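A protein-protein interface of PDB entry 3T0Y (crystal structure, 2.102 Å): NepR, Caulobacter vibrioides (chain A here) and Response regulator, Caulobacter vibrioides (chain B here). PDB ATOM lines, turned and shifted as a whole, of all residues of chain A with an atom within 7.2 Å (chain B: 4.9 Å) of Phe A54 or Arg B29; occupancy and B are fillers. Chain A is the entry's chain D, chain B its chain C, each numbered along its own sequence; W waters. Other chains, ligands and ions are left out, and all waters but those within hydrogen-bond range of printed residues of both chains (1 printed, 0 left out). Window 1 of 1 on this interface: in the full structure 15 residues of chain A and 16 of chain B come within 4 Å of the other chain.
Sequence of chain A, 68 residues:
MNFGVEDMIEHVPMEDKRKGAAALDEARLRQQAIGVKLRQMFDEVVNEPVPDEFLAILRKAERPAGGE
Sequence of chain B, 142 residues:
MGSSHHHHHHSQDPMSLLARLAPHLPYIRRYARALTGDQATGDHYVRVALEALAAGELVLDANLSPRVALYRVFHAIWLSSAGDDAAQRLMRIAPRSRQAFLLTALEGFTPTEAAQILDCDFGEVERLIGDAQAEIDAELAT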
ATOM      1  N   PHE A  42     -28.694   2.979  -2.378  1.00  0.00           N
ATOM      2  CA  PHE A  42     -27.459   2.173  -2.270  1.00  0.00           C
ATOM      3  C   PHE A  42     -27.555   0.794  -1.626  1.00  0.00           C
ATOM      4  O   PHE A  42     -26.612   0.000  -1.736  1.00  0.00           O
ATOM      5  CB  PHE A  42     -26.378   2.949  -1.516  1.00  0.00           C
ATOM      6  CG  PHE A  42     -26.046   4.263  -2.129  1.00  0.00           C
ATOM      7  CD1 PHE A  42     -25.707   4.349  -3.465  1.00  0.00           C
ATOM      8  CD2 PHE A  42     -26.094   5.420  -1.371  1.00  0.00           C
ATOM      9  CE1 PHE A  42     -25.404   5.571  -4.033  1.00  0.00           C
ATOM     10  CE2 PHE A  42     -25.796   6.640  -1.932  1.00  0.00           C
ATOM     11  CZ  PHE A  42     -25.452   6.718  -3.267  1.00  0.00           C
ATOM     12  N   VAL A  45     -27.031  -3.240  -3.401  1.00  0.00           N
ATOM     13  CA  VAL A  45     -25.740  -3.906  -3.518  1.00  0.00           C
ATOM     14  C   VAL A  45     -25.619  -5.069  -2.546  1.00  0.00           C
ATOM     15  O   VAL A  45     -25.071  -6.124  -2.867  1.00  0.00           O
ATOM     16  CB  VAL A  45     -24.612  -2.907  -3.205  1.00  0.00           C
ATOM     17  CG1 VAL A  45     -23.241  -3.571  -3.310  1.00  0.00           C
ATOM     18  CG2 VAL A  45     -24.709  -1.716  -4.136  1.00  0.00           C
ATOM     19  N   VAL A  46     -26.137  -4.851  -1.348  1.00  0.00           N
ATOM     20  CA  VAL A  46     -25.958  -5.777  -0.247  1.00  0.00           C
ATOM     21  C   VAL A  46     -26.601  -7.142  -0.529  1.00  0.00           C
ATOM     22  O   VAL A  46     -26.089  -8.183  -0.101  1.00  0.00           O
ATOM     23  CB  VAL A  46     -26.490  -5.150   1.059  1.00  0.00           C
ATOM     24  CG1 VAL A  46     -26.779  -6.205   2.097  1.00  0.00           C
ATOM     25  CG2 VAL A  46     -25.486  -4.143   1.589  1.00  0.00           C
ATOM     26  N   ASN A  47     -27.707  -7.136  -1.271  1.00  0.00           N
ATOM     27  CA  ASN A  47     -28.405  -8.378  -1.584  1.00  0.00           C
ATOM     28  C   ASN A  47     -27.937  -8.999  -2.895  1.00  0.00           C
ATOM     29  O   ASN A  47     -28.534  -9.958  -3.386  1.00  0.00           O
ATOM     30  CB  ASN A  47     -29.918  -8.170  -1.580  1.00  0.00           C
ATOM     31  CG  ASN A  47     -30.396  -7.482  -0.326  1.00  0.00           C
ATOM     32  OD1 ASN A  47     -30.331  -8.049   0.765  1.00  0.00           O
ATOM     33  ND2 ASN A  47     -30.866  -6.244  -0.467  1.00  0.00           N
ATOM     34  N   GLU A  48     -26.863  -8.448  -3.454  1.00  0.00           N
ATOM     35  CA  GLU A  48     -26.207  -9.049  -4.610  1.00  0.00           C
ATOM     36  C   GLU A  48     -25.144 -10.023  -4.149  1.00  0.00           C
ATOM     37  O   GLU A  48     -24.600  -9.880  -3.054  1.00  0.00           O
ATOM     38  CB  GLU A  48     -25.550  -7.982  -5.476  1.00  0.00           C
ATOM     39  CG  GLU A  48     -26.509  -6.972  -6.060  1.00  0.00           C
ATOM     40  CD  GLU A  48     -25.795  -5.987  -6.948  1.00  0.00           C
ATOM     41  OE1 GLU A  48     -24.693  -6.340  -7.433  1.00  0.00           O
ATOM     42  OE2 GLU A  48     -26.318  -4.865  -7.149  1.00  0.00           O
ATOM     43  N   PRO A  49     -24.846 -11.022  -4.986  1.00  0.00           N
ATOM     44  CA  PRO A  49     -23.778 -11.990  -4.724  1.00  0.00           C
ATOM     45  C   PRO A  49     -22.404 -11.405  -5.017  1.00  0.00           C
ATOM     46  O   PRO A  49     -22.182 -10.781  -6.059  1.00  0.00           O
ATOM     47  CB  PRO A  49     -24.076 -13.117  -5.718  1.00  0.00           C
ATOM     48  CG  PRO A  49     -24.761 -12.423  -6.857  1.00  0.00           C
ATOM     49  CD  PRO A  49     -25.573 -11.313  -6.236  1.00  0.00           C
ATOM     50  N   VAL A  50     -21.486 -11.626  -4.091  1.00  0.00           N
ATOM     51  CA  VAL A  50     -20.126 -11.148  -4.230  1.00  0.00           C
ATOM     52  C   VAL A  50     -19.458 -11.760  -5.444  1.00  0.00           C
ATOM     53  O   VAL A  50     -19.702 -12.916  -5.780  1.00  0.00           O
ATOM     54  CB  VAL A  50     -19.292 -11.506  -2.981  1.00  0.00           C
ATOM     55  CG1 VAL A  50     -17.830 -11.142  -3.181  1.00  0.00           C
ATOM     56  CG2 VAL A  50     -19.863 -10.820  -1.760  1.00  0.00           C
ATOM     57  N   PRO A  51     -18.609 -10.981  -6.117  1.00  0.00           N
ATOM     58  CA  PRO A  51     -17.778 -11.574  -7.169  1.00  0.00           C
ATOM     59  C   PRO A  51     -16.857 -12.660  -6.606  1.00  0.00           C
ATOM     60  O   PRO A  51     -16.259 -12.479  -5.546  1.00  0.00           O
ATOM     61  CB  PRO A  51     -16.956 -10.384  -7.667  1.00  0.00           C
ATOM     62  CG  PRO A  51     -17.811  -9.172  -7.346  1.00  0.00           C
ATOM     63  CD  PRO A  51     -18.466  -9.514  -6.043  1.00  0.00           C
ATOM     64  N   ASP A  52     -16.744 -13.780  -7.313  1.00  0.00           N
ATOM     65  CA  ASP A  52     -15.849 -14.847  -6.887  1.00  0.00           C
ATOM     66  C   ASP A  52     -14.398 -14.389  -6.864  1.00  0.00           C
ATOM     67  O   ASP A  52     -13.586 -14.891  -6.083  1.00  0.00           O
ATOM     68  CB  ASP A  52     -15.994 -16.074  -7.793  1.00  0.00           C
ATOM     69  CG  ASP A  52     -17.279 -16.816  -7.544  1.00  0.00           C
ATOM     70  OD1 ASP A  52     -17.315 -17.641  -6.598  1.00  0.00           O
ATOM     71  OD2 ASP A  52     -18.254 -16.557  -8.281  1.00  0.00           O
ATOM     72  N   GLU A  53     -14.074 -13.439  -7.727  1.00  0.00           N
ATOM     73  CA  GLU A  53     -12.734 -12.890  -7.755  1.00  0.00           C
ATOM     74  C   GLU A  53     -12.367 -12.337  -6.376  1.00  0.00           C
ATOM     75  O   GLU A  53     -11.187 -12.335  -5.994  1.00  0.00           O
ATOM     76  CB  GLU A  53     -12.621 -11.817  -8.844  1.00  0.00           C
ATOM     77  CG  GLU A  53     -11.366 -10.945  -8.774  1.00  0.00           C
ATOM     78  CD  GLU A  53     -10.055 -11.736  -8.832  1.00  0.00           C
ATOM     79  OE1 GLU A  53     -10.098 -12.991  -8.822  1.00  0.00           O
ATOM     80  OE2 GLU A  53      -8.975 -11.093  -8.891  1.00  0.00           O
ATOM     81  N   PHE A  54     -13.373 -11.889  -5.618  1.00  0.00           N
ATOM     82  CA  PHE A  54     -13.107 -11.366  -4.278  1.00  0.00           C
ATOM     83  C   PHE A  54     -12.636 -12.503  -3.380  1.00  0.00           C
ATOM     84  O   PHE A  54     -11.575 -12.416  -2.741  1.00  0.00           O
ATOM     85  CB  PHE A  54     -14.342 -10.698  -3.655  1.00  0.00           C
ATOM     86  CG  PHE A  54     -14.676  -9.342  -4.230  1.00  0.00           C
ATOM     87  CD1 PHE A  54     -14.014  -8.857  -5.343  1.00  0.00           C
ATOM     88  CD2 PHE A  54     -15.653  -8.553  -3.639  1.00  0.00           C
ATOM     89  CE1 PHE A  54     -14.329  -7.620  -5.872  1.00  0.00           C
ATOM     90  CE2 PHE A  54     -15.978  -7.303  -4.159  1.00  0.00           C
ATOM     91  CZ  PHE A  54     -15.317  -6.841  -5.284  1.00  0.00           C
ATOM     92  N   LEU A  55     -13.447 -13.560  -3.327  1.00  0.00           N
ATOM     93  CA  LEU A  55     -13.092 -14.770  -2.589  1.00  0.00           C
ATOM     94  C   LEU A  55     -11.766 -15.303  -3.105  1.00  0.00           C
ATOM     95  O   LEU A  55     -10.873 -15.635  -2.321  1.00  0.00           O
ATOM     96  CB  LEU A  55     -14.172 -15.842  -2.740  1.00  0.00           C
ATOM     97  CG  LEU A  55     -15.613 -15.482  -2.370  1.00  0.00           C
ATOM     98  CD1 LEU A  55     -16.385 -16.752  -2.050  1.00  0.00           C
ATOM     99  CD2 LEU A  55     -15.640 -14.545  -1.185  1.00  0.00           C
ATOM    100  N   ALA A  56     -11.637 -15.366  -4.427  1.00  0.00           N
ATOM    101  CA  ALA A  56     -10.405 -15.833  -5.047  1.00  0.00           C
ATOM    102  C   ALA A  56      -9.217 -15.197  -4.348  1.00  0.00           C
ATOM    103  O   ALA A  56      -8.303 -15.887  -3.898  1.00  0.00           O
ATOM    104  CB  ALA A  56     -10.385 -15.488  -6.532  1.00  0.00           C
ATOM    105  N   ILE A  57      -9.251 -13.875  -4.242  1.00  0.00           N
ATOM    106  CA  ILE A  57      -8.146 -13.131  -3.650  1.00  0.00           C
ATOM    107  C   ILE A  57      -7.880 -13.554  -2.211  1.00  0.00           C
ATOM    108  O   ILE A  57      -6.724 -13.672  -1.791  1.00  0.00           O
ATOM    109  CB  ILE A  57      -8.397 -11.612  -3.702  1.00  0.00           C
ATOM    110  CG1 ILE A  57      -8.633 -11.175  -5.147  1.00  0.00           C
ATOM    111  CG2 ILE A  57      -7.223 -10.853  -3.100  1.00  0.00           C
ATOM    112  CD1 ILE A  57      -8.419  -9.710  -5.377  1.00  0.00           C
ATOM    113  N   LEU A  58      -8.954 -13.797  -1.465  1.00  0.00           N
ATOM    114  CA  LEU A  58      -8.842 -14.097  -0.045  1.00  0.00           C
ATOM    115  C   LEU A  58      -8.431 -15.545   0.216  1.00  0.00           C
ATOM    116  O   LEU A  58      -7.635 -15.811   1.131  1.00  0.00           O
ATOM    117  CB  LEU A  58     -10.150 -13.765   0.685  1.00  0.00           C
ATOM    118  CG  LEU A  58     -10.446 -12.269   0.814  1.00  0.00           C
ATOM    119  CD1 LEU A  58     -11.830 -12.040   1.402  1.00  0.00           C
ATOM    120  CD2 LEU A  58      -9.370 -11.571   1.640  1.00  0.00           C
ATOM    121  N   ARG A  59      -8.977 -16.472  -0.578  1.00  0.00           N
ATOM    122  CA  ARG A  59      -8.666 -17.896  -0.442  1.00  0.00           C
ATOM    123  C   ARG A  59      -7.154 -18.098  -0.404  1.00  0.00           C
ATOM    124  O   ARG A  59      -6.635 -18.893   0.385  1.00  0.00           O
ATOM    125  CB  ARG A  59      -9.258 -18.711  -1.601  1.00  0.00           C
ATOM    126  CG  ARG A  59     -10.778 -18.626  -1.781  1.00  0.00           C
ATOM    127  CD  ARG A  59     -11.278 -19.752  -2.694  1.00  0.00           C
ATOM    128  NE  ARG A  59     -12.078 -19.284  -3.826  1.00  0.00           N
ATOM    129  CZ  ARG A  59     -13.408 -19.266  -3.849  1.00  0.00           C
ATOM    130  NH1 ARG A  59     -14.100 -19.687  -2.795  1.00  0.00           N
ATOM    131  NH2 ARG A  59     -14.048 -18.824  -4.925  1.00  0.00           N
ATOM    132  N   LEU B  25     -18.209  -8.601   2.987  1.00  0.00           N
ATOM    133  CA  LEU B  25     -17.935  -8.194   1.607  1.00  0.00           C
ATOM    134  C   LEU B  25     -19.107  -7.494   0.906  1.00  0.00           C
ATOM    135  O   LEU B  25     -18.891  -6.534   0.185  1.00  0.00           O
ATOM    136  CB  LEU B  25     -17.385  -9.368   0.767  1.00  0.00           C
ATOM    137  CG  LEU B  25     -16.038  -9.967   1.219  1.00  0.00           C
ATOM    138  CD1 LEU B  25     -15.530 -11.026   0.242  1.00  0.00           C
ATOM    139  CD2 LEU B  25     -14.957  -8.905   1.450  1.00  0.00           C
ATOM    140  N   PRO B  26     -20.347  -7.963   1.107  1.00  0.00           N
ATOM    141  CA  PRO B  26     -21.452  -7.228   0.475  1.00  0.00           C
ATOM    142  C   PRO B  26     -21.543  -5.793   0.991  1.00  0.00           C
ATOM    143  O   PRO B  26     -22.014  -4.906   0.272  1.00  0.00           O
ATOM    144  CB  PRO B  26     -22.706  -8.012   0.910  1.00  0.00           C
ATOM    145  CG  PRO B  26     -22.213  -9.365   1.285  1.00  0.00           C
ATOM    146  CD  PRO B  26     -20.816  -9.159   1.828  1.00  0.00           C
ATOM    147  N   TYR B  27     -21.109  -5.562   2.227  1.00  0.00           N
ATOM    148  CA  TYR B  27     -21.232  -4.231   2.822  1.00  0.00           C
ATOM    149  C   TYR B  27     -20.147  -3.279   2.345  1.00  0.00           C
ATOM    150  O   TYR B  27     -20.442  -2.168   1.951  1.00  0.00           O
ATOM    151  CB  TYR B  27     -21.297  -4.331   4.338  1.00  0.00           C
ATOM    152  CG  TYR B  27     -22.472  -5.180   4.720  1.00  0.00           C
ATOM    153  CD1 TYR B  27     -23.747  -4.631   4.787  1.00  0.00           C
ATOM    154  CD2 TYR B  27     -22.330  -6.542   4.933  1.00  0.00           C
ATOM    155  CE1 TYR B  27     -24.837  -5.403   5.097  1.00  0.00           C
ATOM    156  CE2 TYR B  27     -23.422  -7.332   5.246  1.00  0.00           C
ATOM    157  CZ  TYR B  27     -24.673  -6.754   5.328  1.00  0.00           C
ATOM    158  OH  TYR B  27     -25.768  -7.522   5.633  1.00  0.00           O
ATOM    159  N   ILE B  28     -18.906  -3.742   2.313  1.00  0.00           N
ATOM    160  CA  ILE B  28     -17.844  -2.939   1.765  1.00  0.00           C
ATOM    161  C   ILE B  28     -18.160  -2.619   0.302  1.00  0.00           C
ATOM    162  O   ILE B  28     -17.805  -1.551  -0.191  1.00  0.00           O
ATOM    163  CB  ILE B  28     -16.446  -3.604   1.957  1.00  0.00           C
ATOM    164  CG1 ILE B  28     -15.324  -2.581   1.787  1.00  0.00           C
ATOM    165  CG2 ILE B  28     -16.241  -4.768   1.012  1.00  0.00           C
ATOM    166  CD1 ILE B  28     -15.502  -1.358   2.648  1.00  0.00           C
ATOM    167  N   ARG B  29     -18.871  -3.501  -0.397  1.00  0.00           N
ATOM    168  CA  ARG B  29     -19.176  -3.181  -1.793  1.00  0.00           C
ATOM    169  C   ARG B  29     -20.165  -2.050  -1.851  1.00  0.00           C
ATOM    170  O   ARG B  29     -20.088  -1.196  -2.743  1.00  0.00           O
ATOM    171  CB  ARG B  29     -19.760  -4.363  -2.561  1.00  0.00           C
ATOM    172  CG  ARG B  29     -18.855  -5.547  -2.716  1.00  0.00           C
ATOM    173  CD  ARG B  29     -19.557  -6.610  -3.573  1.00  0.00           C
ATOM    174  NE  ARG B  29     -19.561  -6.269  -4.997  1.00  0.00           N
ATOM    175  CZ  ARG B  29     -20.550  -6.549  -5.841  1.00  0.00           C
ATOM    176  NH1 ARG B  29     -21.646  -7.160  -5.403  1.00  0.00           N
ATOM    177  NH2 ARG B  29     -20.449  -6.205  -7.124  1.00  0.00           N
ATOM    178  N   ARG B  30     -21.120  -2.062  -0.922  1.00  0.00           N
ATOM    179  CA  ARG B  30     -22.105  -0.997  -0.877  1.00  0.00           C
ATOM    180  C   ARG B  30     -21.382   0.318  -0.628  1.00  0.00           C
ATOM    181  O   ARG B  30     -21.639   1.304  -1.300  1.00  0.00           O
ATOM    182  CB  ARG B  30     -23.153  -1.229   0.217  1.00  0.00           C
ATOM    183  CG  ARG B  30     -24.153  -0.074   0.334  1.00  0.00           C
ATOM    184  CD  ARG B  30     -25.060  -0.216   1.536  1.00  0.00           C
ATOM    185  NE  ARG B  30     -24.275  -0.430   2.738  1.00  0.00           N
ATOM    186  CZ  ARG B  30     -24.764  -0.824   3.902  1.00  0.00           C
ATOM    187  NH1 ARG B  30     -26.064  -1.062   4.037  1.00  0.00           N
ATOM    188  NH2 ARG B  30     -23.940  -1.013   4.919  1.00  0.00           N
ATOM    189  N   TYR B  31     -20.475   0.326   0.344  1.00  0.00           N
ATOM    190  CA  TYR B  31     -19.785   1.558   0.698  1.00  0.00           C
ATOM    191  C   TYR B  31     -18.935   2.033  -0.483  1.00  0.00           C
ATOM    192  O   TYR B  31     -18.966   3.206  -0.854  1.00  0.00           O
ATOM    193  CB  TYR B  31     -18.917   1.339   1.928  1.00  0.00           C
ATOM    194  CG  TYR B  31     -18.035   2.509   2.259  1.00  0.00           C
ATOM    195  CD1 TYR B  31     -18.587   3.705   2.703  1.00  0.00           C
ATOM    196  CD2 TYR B  31     -16.650   2.425   2.127  1.00  0.00           C
ATOM    197  CE1 TYR B  31     -17.794   4.791   2.999  1.00  0.00           C
ATOM    198  CE2 TYR B  31     -15.844   3.505   2.429  1.00  0.00           C
ATOM    199  CZ  TYR B  31     -16.435   4.695   2.873  1.00  0.00           C
ATOM    200  OH  TYR B  31     -15.666   5.786   3.203  1.00  0.00           O
ATOM    201  N   ALA B  32     -18.194   1.097  -1.072  1.00  0.00           N
ATOM    202  CA  ALA B  32     -17.283   1.379  -2.167  1.00  0.00           C
ATOM    203  C   ALA B  32     -18.005   2.075  -3.297  1.00  0.00           C
ATOM    204  O   ALA B  32     -17.529   3.091  -3.823  1.00  0.00           O
ATOM    205  CB  ALA B  32     -16.643   0.058  -2.662  1.00  0.00           C
ATOM    206  N   ARG B  33     -19.178   1.543  -3.648  1.00  0.00           N
ATOM    207  CA  ARG B  33     -19.971   2.055  -4.761  1.00  0.00           C
ATOM    208  C   ARG B  33     -20.507   3.439  -4.419  1.00  0.00           C
ATOM    209  O   ARG B  33     -20.497   4.336  -5.254  1.00  0.00           O
ATOM    210  CB  ARG B  33     -21.085   1.056  -5.135  1.00  0.00           C
ATOM    211  CG  ARG B  33     -22.539   1.585  -5.270  1.00  0.00           C
ATOM    212  CD  ARG B  33     -22.723   2.583  -6.402  1.00  0.00           C
ATOM    213  NE  ARG B  33     -23.993   2.552  -7.153  1.00  0.00           N
ATOM    214  CZ  ARG B  33     -25.085   1.826  -6.879  1.00  0.00           C
ATOM    215  NH1 ARG B  33     -25.149   1.028  -5.820  1.00  0.00           N
ATOM    216  NH2 ARG B  33     -26.143   1.916  -7.685  1.00  0.00           N
ATOM    217  N   GLN B  39     -20.400   0.649  -9.276  1.00  0.00           N
ATOM    218  CA  GLN B  39     -19.982  -0.643  -8.741  1.00  0.00           C
ATOM    219  C   GLN B  39     -18.640  -1.075  -9.310  1.00  0.00           C
ATOM    220  O   GLN B  39     -17.846  -1.703  -8.616  1.00  0.00           O
ATOM    221  CB  GLN B  39     -21.039  -1.723  -9.018  1.00  0.00           C
ATOM    222  CG  GLN B  39     -20.983  -2.904  -8.045  1.00  0.00           C
ATOM    223  CD  GLN B  39     -21.204  -2.467  -6.586  1.00  0.00           C
ATOM    224  OE1 GLN B  39     -22.334  -2.160  -6.181  1.00  0.00           O
ATOM    225  NE2 GLN B  39     -20.114  -2.422  -5.798  1.00  0.00           N
ATOM    226  N   ASP B  43     -15.770  -1.893  -6.849  1.00  0.00           N
ATOM    227  CA  ASP B  43     -15.147  -3.206  -6.870  1.00  0.00           C
ATOM    228  C   ASP B  43     -13.661  -3.114  -7.169  1.00  0.00           C
ATOM    229  O   ASP B  43     -12.882  -3.911  -6.678  1.00  0.00           O
ATOM    230  CB  ASP B  43     -15.839  -4.120  -7.881  1.00  0.00           C
ATOM    231  CG  ASP B  43     -17.253  -4.472  -7.464  1.00  0.00           C
ATOM    232  OD1 ASP B  43     -17.613  -4.149  -6.319  1.00  0.00           O
ATOM    233  OD2 ASP B  43     -18.001  -5.090  -8.255  1.00  0.00           O
ATOM    234  N   VAL B  46     -12.173  -2.298  -3.704  1.00  0.00           N
ATOM    235  CA  VAL B  46     -12.281  -3.456  -2.855  1.00  0.00           C
ATOM    236  C   VAL B  46     -11.207  -4.499  -3.214  1.00  0.00           C
ATOM    237  O   VAL B  46     -10.563  -5.071  -2.326  1.00  0.00           O
ATOM    238  CB  VAL B  46     -13.690  -4.096  -2.956  1.00  0.00           C
ATOM    239  CG1 VAL B  46     -13.761  -5.308  -2.056  1.00  0.00           C
ATOM    240  CG2 VAL B  46     -14.764  -3.072  -2.588  1.00  0.00           C
ATOM    241  N   ARG B  47     -11.041  -4.769  -4.514  1.00  0.00           N
ATOM    242  CA  ARG B  47     -10.052  -5.749  -4.954  1.00  0.00           C
ATOM    243  C   ARG B  47      -8.672  -5.324  -4.481  1.00  0.00           C
ATOM    244  O   ARG B  47      -7.958  -6.093  -3.858  1.00  0.00           O
ATOM    245  CB  ARG B  47     -10.065  -5.933  -6.482  1.00  0.00           C
ATOM    246  CG  ARG B  47     -11.197  -6.826  -7.000  1.00  0.00           C
ATOM    247  CD  ARG B  47     -10.968  -7.267  -8.465  1.00  0.00           C
ATOM    248  NE  ARG B  47     -10.658  -6.131  -9.326  1.00  0.00           N
ATOM    249  CZ  ARG B  47     -11.569  -5.391  -9.949  1.00  0.00           C
ATOM    250  NH1 ARG B  47     -12.860  -5.680  -9.828  1.00  0.00           N
ATOM    251  NH2 ARG B  47     -11.190  -4.360 -10.695  1.00  0.00           N
ATOM    252  N   LEU B  50      -8.294  -6.090  -0.796  1.00  0.00           N
ATOM    253  CA  LEU B  50      -8.200  -7.487  -0.440  1.00  0.00           C
ATOM    254  C   LEU B  50      -6.845  -8.030  -0.857  1.00  0.00           C
ATOM    255  O   LEU B  50      -6.322  -8.949  -0.239  1.00  0.00           O
ATOM    256  CB  LEU B  50      -9.325  -8.288  -1.096  1.00  0.00           C
ATOM    257  CG  LEU B  50     -10.698  -7.788  -0.649  1.00  0.00           C
ATOM    258  CD1 LEU B  50     -11.817  -8.486  -1.392  1.00  0.00           C
ATOM    259  CD2 LEU B  50     -10.838  -7.984   0.844  1.00  0.00           C
HETATM  260  O   HOH W   1     -22.435  -7.891  -2.873  1.00  0.00           O
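The guanidinium group (NH1) of Arg B29 lies within salt-bridge range of the side-chain carboxylate (OE1) of Glu A48 (3.8 Å).
The guanidinium group (NH2) of Arg B29 is in salt-bridge range of the side-chain carboxylate (OD2) of Asp B43, at 2.9 Å. The side-chain carboxylate (OD1) of Asp B43 lies within hydrogen-bond range of the side-chain amide nitrogen (NE2) of Gln B39. The backbone carbonyl oxygen (O) of Arg B29 sits at hydrogen-bond distance from the side-chain amide nitrogen (NE2) of Gln B39 (3.3 Å).
Among the printed residues, pairs that only touch across the chains: Val A45 with Gln B39 (3.2 Å), Phe A42 with Arg B30 (3.2 Å), Val A45 with Arg B33 (3.2 Å), Phe A54 with Arg B47 (3.4 Å), Val A45 with Arg B30 (3.5 Å), Val A46 with Pro B26 (3.5 Å), Ile A57 with Leu B50 (3.6 Å), Pro A51 with Arg B29 (3.6 Å), Val A45 with Arg B29 (3.6 Å), Phe A54 with Val B46 (3.6 Å), Val A46 with Tyr B27 (3.7 Å), Phe A54 with Arg B29 (3.7 Å), Phe A54 with Asp B43 (3.7 Å), Glu A53 with Arg B47 (3.7 Å), Pro A49 with Arg B29 (3.7 Å), Leu A55 with Leu B25 (3.8 Å), Val A50 with Leu B25 (3.8 Å), Ile A57 with Arg B47 (3.95 Å), Val A46 with Arg B30 (3.95 Å) and Leu A58 with Leu B50 (3.96 Å).
Of the printed residues of chain B, Phe A42 touches Arg B30 (3.2 Å). Asn A47 touches none of the printed residues of chain B. Printed residues of chain B within 4 Å of Glu A48: Arg B29 (3.8 Å). Of chain B, only Arg B29 (3.7 Å), Asp B43 (3.7 Å), Val B46 (3.6 Å) and Arg B47 (3.4 Å) come within 4 Å of Phe A54. Ala A56 touches none of the printed residues of chain B. Of chain A, only Val A45, Glu A48, Pro A49, Pro A51 and Phe A54 come within 4 Å of Arg B29. The nearest residue of chain A that does not touch Arg B29 is Val A50 (4.4 Å). The nearest printed residue of chain B that does not touch Val A50 is Pro B26 (4.1 Å).
Printed residues of chain A that touch a printed residue of chain B: Phe A42, Val A45, Val A46, Glu A48, Pro A49, Val A50, Pro A51, Glu A53, Phe A54, Leu A55, Ile A57 and Leu A58. Along chain A the printed residues that touch a printed residue of chain B span positions 42 to 58. Printed residues of chain B that touch a printed residue of chain A: Leu B25, Pro B26, Tyr B27, Arg B29, Arg B30, Arg B33, Gln B39, Asp B43, Val B46, Arg B47 and Leu B50. Hydrophobic or aromatic side chains of chain B that line the printed part of chain A: Leu B25, Pro B26, Tyr B27, Val B46 and Leu B50. Among the printed residues, Asp or Glu carboxylates within 4 Å of a Lys or Arg side-chain nitrogen of the other chain: Glu A48 with Arg B29.
Water W1 lies within hydrogen-bond range of NH1 of Arg B29 (2.7 Å), O of Glu A48 (2.9 Å) and O of Val A45 (3.2 Å).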
